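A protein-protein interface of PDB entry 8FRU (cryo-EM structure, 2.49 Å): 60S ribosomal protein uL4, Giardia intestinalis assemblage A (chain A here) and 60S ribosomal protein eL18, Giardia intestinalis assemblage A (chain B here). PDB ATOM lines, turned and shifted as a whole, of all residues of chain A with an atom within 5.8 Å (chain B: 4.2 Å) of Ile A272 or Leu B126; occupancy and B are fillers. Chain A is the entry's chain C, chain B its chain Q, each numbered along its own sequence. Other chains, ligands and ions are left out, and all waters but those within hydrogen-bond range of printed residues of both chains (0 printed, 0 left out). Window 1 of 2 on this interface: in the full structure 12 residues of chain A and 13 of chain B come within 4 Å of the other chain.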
ATOM      1  N   ILE A 264      -6.179  17.650 -12.888  1.00  0.00           N
ATOM      2  CA  ILE A 264      -5.635  16.391 -13.378  1.00  0.00           C
ATOM      3  C   ILE A 264      -5.332  15.459 -12.208  1.00  0.00           C
ATOM      4  O   ILE A 264      -5.181  15.883 -11.060  1.00  0.00           O
ATOM      5  CB  ILE A 264      -4.378  16.634 -14.226  1.00  0.00           C
ATOM      6  CG1 ILE A 264      -3.285  17.268 -13.365  1.00  0.00           C
ATOM      7  CG2 ILE A 264      -4.701  17.513 -15.416  1.00  0.00           C
ATOM      8  CD1 ILE A 264      -1.894  16.976 -13.848  1.00  0.00           C
ATOM      9  N   ASP A 268      -2.924  10.911 -15.315  1.00  0.00           N
ATOM     10  CA  ASP A 268      -2.742  11.869 -16.392  1.00  0.00           C
ATOM     11  C   ASP A 268      -1.358  12.500 -16.395  1.00  0.00           C
ATOM     12  O   ASP A 268      -1.024  13.206 -17.351  1.00  0.00           O
ATOM     13  CB  ASP A 268      -3.809  12.961 -16.295  1.00  0.00           C
ATOM     14  CG  ASP A 268      -5.037  12.512 -15.514  1.00  0.00           C
ATOM     15  OD1 ASP A 268      -5.128  11.311 -15.187  1.00  0.00           O
ATOM     16  OD2 ASP A 268      -5.910  13.358 -15.228  1.00  0.00           O
ATOM     17  N   ILE A 269      -0.551  12.267 -15.365  1.00  0.00           N
ATOM     18  CA  ILE A 269       0.752  12.916 -15.262  1.00  0.00           C
ATOM     19  C   ILE A 269       1.831  12.119 -15.983  1.00  0.00           C
ATOM     20  O   ILE A 269       2.626  12.683 -16.739  1.00  0.00           O
ATOM     21  CB  ILE A 269       1.118  13.153 -13.782  1.00  0.00           C
ATOM     22  CG1 ILE A 269       2.240  14.180 -13.667  1.00  0.00           C
ATOM     23  CG2 ILE A 269       1.551  11.868 -13.119  1.00  0.00           C
ATOM     24  CD1 ILE A 269       1.748  15.569 -13.380  1.00  0.00           C
ATOM     25  N   GLU A 270       1.898  10.802 -15.774  1.00  0.00           N
ATOM     26  CA  GLU A 270       2.922  10.036 -16.474  1.00  0.00           C
ATOM     27  C   GLU A 270       2.655   9.960 -17.966  1.00  0.00           C
ATOM     28  O   GLU A 270       3.593   9.754 -18.738  1.00  0.00           O
ATOM     29  CB  GLU A 270       3.062   8.621 -15.911  1.00  0.00           C
ATOM     30  CG  GLU A 270       1.801   7.803 -15.872  1.00  0.00           C
ATOM     31  CD  GLU A 270       0.882   8.242 -14.767  1.00  0.00           C
ATOM     32  OE1 GLU A 270       1.283   9.138 -14.001  1.00  0.00           O
ATOM     33  OE2 GLU A 270      -0.220   7.675 -14.649  1.00  0.00           O
ATOM     34  N   ARG A 271       1.406  10.128 -18.393  1.00  0.00           N
ATOM     35  CA  ARG A 271       1.157  10.262 -19.821  1.00  0.00           C
ATOM     36  C   ARG A 271       1.880  11.479 -20.377  1.00  0.00           C
ATOM     37  O   ARG A 271       2.524  11.403 -21.427  1.00  0.00           O
ATOM     38  CB  ARG A 271      -0.342  10.353 -20.089  1.00  0.00           C
ATOM     39  CG  ARG A 271      -0.747   9.838 -21.456  1.00  0.00           C
ATOM     40  CD  ARG A 271      -2.153  10.265 -21.805  1.00  0.00           C
ATOM     41  NE  ARG A 271      -2.516  11.511 -21.143  1.00  0.00           N
ATOM     42  CZ  ARG A 271      -3.494  11.631 -20.256  1.00  0.00           C
ATOM     43  NH1 ARG A 271      -4.238  10.595 -19.903  1.00  0.00           N
ATOM     44  NH2 ARG A 271      -3.731  12.818 -19.709  1.00  0.00           N
ATOM     45  N   ILE A 272       1.802  12.607 -19.670  1.00  0.00           N
ATOM     46  CA  ILE A 272       2.520  13.806 -20.089  1.00  0.00           C
ATOM     47  C   ILE A 272       4.022  13.576 -20.031  1.00  0.00           C
ATOM     48  O   ILE A 272       4.761  13.963 -20.942  1.00  0.00           O
ATOM     49  CB  ILE A 272       2.107  15.006 -19.221  1.00  0.00           C
ATOM     50  CG1 ILE A 272       0.713  15.495 -19.604  1.00  0.00           C
ATOM     51  CG2 ILE A 272       3.131  16.122 -19.336  1.00  0.00           C
ATOM     52  CD1 ILE A 272       0.210  16.600 -18.723  1.00  0.00           C
ATOM     53  N   LEU A 273       4.498  12.951 -18.955  1.00  0.00           N
ATOM     54  CA  LEU A 273       5.934  12.794 -18.769  1.00  0.00           C
ATOM     55  C   LEU A 273       6.547  11.795 -19.739  1.00  0.00           C
ATOM     56  O   LEU A 273       7.757  11.854 -19.978  1.00  0.00           O
ATOM     57  CB  LEU A 273       6.241  12.373 -17.334  1.00  0.00           C
ATOM     58  CG  LEU A 273       6.469  13.513 -16.343  1.00  0.00           C
ATOM     59  CD1 LEU A 273       6.890  12.976 -14.988  1.00  0.00           C
ATOM     60  CD2 LEU A 273       7.504  14.481 -16.878  1.00  0.00           C
ATOM     61  N   GLN A 274       5.758  10.880 -20.293  1.00  0.00           N
ATOM     62  CA  GLN A 274       6.270   9.890 -21.229  1.00  0.00           C
ATOM     63  C   GLN A 274       6.096  10.302 -22.682  1.00  0.00           C
ATOM     64  O   GLN A 274       6.415   9.515 -23.575  1.00  0.00           O
ATOM     65  CB  GLN A 274       5.603   8.532 -20.987  1.00  0.00           C
ATOM     66  CG  GLN A 274       6.076   7.862 -19.705  1.00  0.00           C
ATOM     67  CD  GLN A 274       5.371   6.549 -19.416  1.00  0.00           C
ATOM     68  OE1 GLN A 274       4.816   6.354 -18.335  1.00  0.00           O
ATOM     69  NE2 GLN A 274       5.409   5.631 -20.377  1.00  0.00           N
ATOM     70  N   SER A 275       5.607  11.508 -22.942  1.00  0.00           N
ATOM     71  CA  SER A 275       5.439  11.977 -24.307  1.00  0.00           C
ATOM     72  C   SER A 275       6.784  12.369 -24.911  1.00  0.00           C
ATOM     73  O   SER A 275       7.780  12.562 -24.211  1.00  0.00           O
ATOM     74  CB  SER A 275       4.480  13.163 -24.355  1.00  0.00           C
ATOM     75  OG  SER A 275       4.796  14.109 -23.353  1.00  0.00           O
ATOM     76  N   VAL A 278       8.273  16.129 -24.074  1.00  0.00           N
ATOM     77  CA  VAL A 278       9.090  16.229 -22.872  1.00  0.00           C
ATOM     78  C   VAL A 278      10.368  15.415 -23.011  1.00  0.00           C
ATOM     79  O   VAL A 278      11.386  15.743 -22.394  1.00  0.00           O
ATOM     80  CB  VAL A 278       8.274  15.792 -21.644  1.00  0.00           C
ATOM     81  CG1 VAL A 278       9.136  15.788 -20.400  1.00  0.00           C
ATOM     82  CG2 VAL A 278       7.088  16.708 -21.456  1.00  0.00           C
ATOM     83  N   ALA B  32       6.740  15.862 -10.489  1.00  0.00           N
ATOM     84  CA  ALA B  32       6.966  15.888 -11.930  1.00  0.00           C
ATOM     85  C   ALA B  32       8.097  16.840 -12.293  1.00  0.00           C
ATOM     86  O   ALA B  32       8.983  16.504 -13.091  1.00  0.00           O
ATOM     87  CB  ALA B  32       5.681  16.272 -12.659  1.00  0.00           C
ATOM     88  N   PHE B  33       8.093  18.039 -11.713  1.00  0.00           N
ATOM     89  CA  PHE B  33       9.142  18.986 -12.066  1.00  0.00           C
ATOM     90  C   PHE B  33      10.490  18.565 -11.501  1.00  0.00           C
ATOM     91  O   PHE B  33      11.528  18.842 -12.114  1.00  0.00           O
ATOM     92  CB  PHE B  33       8.762  20.392 -11.615  1.00  0.00           C
ATOM     93  CG  PHE B  33       7.951  21.139 -12.630  1.00  0.00           C
ATOM     94  CD1 PHE B  33       8.551  21.680 -13.751  1.00  0.00           C
ATOM     95  CD2 PHE B  33       6.582  21.273 -12.481  1.00  0.00           C
ATOM     96  CE1 PHE B  33       7.806  22.357 -14.689  1.00  0.00           C
ATOM     97  CE2 PHE B  33       5.831  21.946 -13.416  1.00  0.00           C
ATOM     98  CZ  PHE B  33       6.441  22.490 -14.521  1.00  0.00           C
ATOM     99  N   VAL B  36      11.770  16.180 -14.116  1.00  0.00           N
ATOM    100  CA  VAL B  36      12.249  16.895 -15.293  1.00  0.00           C
ATOM    101  C   VAL B  36      13.616  17.504 -15.025  1.00  0.00           C
ATOM    102  O   VAL B  36      14.512  17.443 -15.872  1.00  0.00           O
ATOM    103  CB  VAL B  36      11.234  17.963 -15.734  1.00  0.00           C
ATOM    104  CG1 VAL B  36      11.921  19.000 -16.597  1.00  0.00           C
ATOM    105  CG2 VAL B  36      10.104  17.321 -16.492  1.00  0.00           C
ATOM    106  N   PHE B 122      -0.168  24.790 -14.598  1.00  0.00           N
ATOM    107  CA  PHE B 122       1.176  24.231 -14.569  1.00  0.00           C
ATOM    108  C   PHE B 122       1.231  22.882 -15.267  1.00  0.00           C
ATOM    109  O   PHE B 122       2.286  22.486 -15.768  1.00  0.00           O
ATOM    110  CB  PHE B 122       1.663  24.113 -13.128  1.00  0.00           C
ATOM    111  CG  PHE B 122       2.349  25.344 -12.628  1.00  0.00           C
ATOM    112  CD1 PHE B 122       1.622  26.375 -12.067  1.00  0.00           C
ATOM    113  CD2 PHE B 122       3.717  25.482 -12.730  1.00  0.00           C
ATOM    114  CE1 PHE B 122       2.243  27.513 -11.613  1.00  0.00           C
ATOM    115  CE2 PHE B 122       4.343  26.622 -12.273  1.00  0.00           C
ATOM    116  CZ  PHE B 122       3.605  27.635 -11.715  1.00  0.00           C
ATOM    117  N   ASP B 123       0.110  22.165 -15.313  1.00  0.00           N
ATOM    118  CA  ASP B 123       0.058  20.921 -16.071  1.00  0.00           C
ATOM    119  C   ASP B 123       0.304  21.173 -17.554  1.00  0.00           C
ATOM    120  O   ASP B 123       1.105  20.480 -18.194  1.00  0.00           O
ATOM    121  CB  ASP B 123      -1.291  20.242 -15.846  1.00  0.00           C
ATOM    122  CG  ASP B 123      -1.384  18.896 -16.525  1.00  0.00           C
ATOM    123  N   GLU B 124      -0.358  22.183 -18.116  1.00  0.00           N
ATOM    124  CA  GLU B 124      -0.136  22.510 -19.519  1.00  0.00           C
ATOM    125  C   GLU B 124       1.252  23.091 -19.756  1.00  0.00           C
ATOM    126  O   GLU B 124       1.843  22.862 -20.817  1.00  0.00           O
ATOM    127  CB  GLU B 124      -1.223  23.464 -20.011  1.00  0.00           C
ATOM    128  CG  GLU B 124      -2.623  22.895 -19.877  1.00  0.00           C
ATOM    129  CD  GLU B 124      -3.631  23.891 -19.341  1.00  0.00           C
ATOM    130  OE1 GLU B 124      -4.472  24.373 -20.129  1.00  0.00           O
ATOM    131  OE2 GLU B 124      -3.602  24.177 -18.129  1.00  0.00           O
ATOM    132  N   LEU B 125       1.792  23.837 -18.794  1.00  0.00           N
ATOM    133  CA  LEU B 125       3.161  24.319 -18.935  1.00  0.00           C
ATOM    134  C   LEU B 125       4.144  23.160 -18.985  1.00  0.00           C
ATOM    135  O   LEU B 125       5.070  23.154 -19.801  1.00  0.00           O
ATOM    136  CB  LEU B 125       3.513  25.265 -17.789  1.00  0.00           C
ATOM    137  CG  LEU B 125       4.866  25.956 -17.954  1.00  0.00           C
ATOM    138  CD1 LEU B 125       4.717  27.175 -18.833  1.00  0.00           C
ATOM    139  CD2 LEU B 125       5.471  26.324 -16.613  1.00  0.00           C
ATOM    140  N   LEU B 126       3.958  22.168 -18.117  1.00  0.00           N
ATOM    141  CA  LEU B 126       4.797  20.979 -18.160  1.00  0.00           C
ATOM    142  C   LEU B 126       4.635  20.247 -19.484  1.00  0.00           C
ATOM    143  O   LEU B 126       5.614  19.764 -20.060  1.00  0.00           O
ATOM    144  CB  LEU B 126       4.452  20.059 -16.991  1.00  0.00           C
ATOM    145  CG  LEU B 126       5.205  18.736 -16.885  1.00  0.00           C
ATOM    146  CD1 LEU B 126       6.477  18.913 -16.082  1.00  0.00           C
ATOM    147  CD2 LEU B 126       4.323  17.682 -16.262  1.00  0.00           C
ATOM    148  N   ALA B 127       3.403  20.157 -19.982  1.00  0.00           N
ATOM    149  CA  ALA B 127       3.169  19.453 -21.236  1.00  0.00           C
ATOM    150  C   ALA B 127       3.861  20.142 -22.407  1.00  0.00           C
ATOM    151  O   ALA B 127       4.399  19.474 -23.296  1.00  0.00           O
ATOM    152  CB  ALA B 127       1.670  19.329 -21.494  1.00  0.00           C
ATOM    153  N   GLU B 128       3.856  21.475 -22.435  1.00  0.00           N
ATOM    154  CA  GLU B 128       4.346  22.206 -23.598  1.00  0.00           C
ATOM    155  C   GLU B 128       5.786  22.693 -23.463  1.00  0.00           C
ATOM    156  O   GLU B 128       6.588  22.495 -24.379  1.00  0.00           O
ATOM    157  CB  GLU B 128       3.424  23.388 -23.900  1.00  0.00           C
ATOM    158  CG  GLU B 128       1.951  23.050 -23.818  1.00  0.00           C
ATOM    159  CD  GLU B 128       1.071  24.228 -24.160  1.00  0.00           C
ATOM    160  OE1 GLU B 128       0.942  24.540 -25.362  1.00  0.00           O
ATOM    161  OE2 GLU B 128       0.504  24.841 -23.232  1.00  0.00           O
ATOM    162  N   PRO B 130       8.496  22.196 -20.793  1.00  0.00           N
ATOM    163  CA  PRO B 130       9.057  21.682 -19.536  1.00  0.00           C
ATOM    164  C   PRO B 130      10.286  22.438 -19.061  1.00  0.00           C
ATOM    165  O   PRO B 130      10.476  22.586 -17.849  1.00  0.00           O
ATOM    166  CB  PRO B 130       9.385  20.220 -19.868  1.00  0.00           C
ATOM    167  CG  PRO B 130       8.611  19.912 -21.102  1.00  0.00           C
ATOM    168  CD  PRO B 130       8.514  21.189 -21.862  1.00  0.00           C
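Of the printed residues of chain B, Leu A273 touches Val B36.
Of the printed residues of chain A, Asp B123 touches Ile A264 and Ile A272.
Printed residues of chain B within 4 Å of Val A278: Leu B126 (3.7 Å) and Pro B130 (3.6 Å).
Of the printed residues of chain A, Ala B127 touches Ile A272 (3.8 Å).
The nearest printed residue of chain A that does not touch Val B36 is Val A278 (4.3 Å).
Hydrophobic or aromatic side chains of chain B that line the printed part of chain A: Val B36, Leu B126 and Pro B130.
Along chain A the printed residues that touch a printed residue of chain B span positions 264 to 278.
OG of Ser A275 lies within hydrogen-bond range of O of Ile A272 (2.4 Å).
Among the printed residues, pairs that only touch across the chains: Ile A264 with Asp B123 (3.3 Å), Ile A272 with Asp B123 (3.6 Å), Val A278 with Pro B130 (3.6 Å), Ile A272 with Leu B126 (3.6 Å), Val A278 with Leu B126 (3.7 Å), Ile A272 with Ala B127 (3.8 Å) and Leu A273 with Val B36 (3.9 Å).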
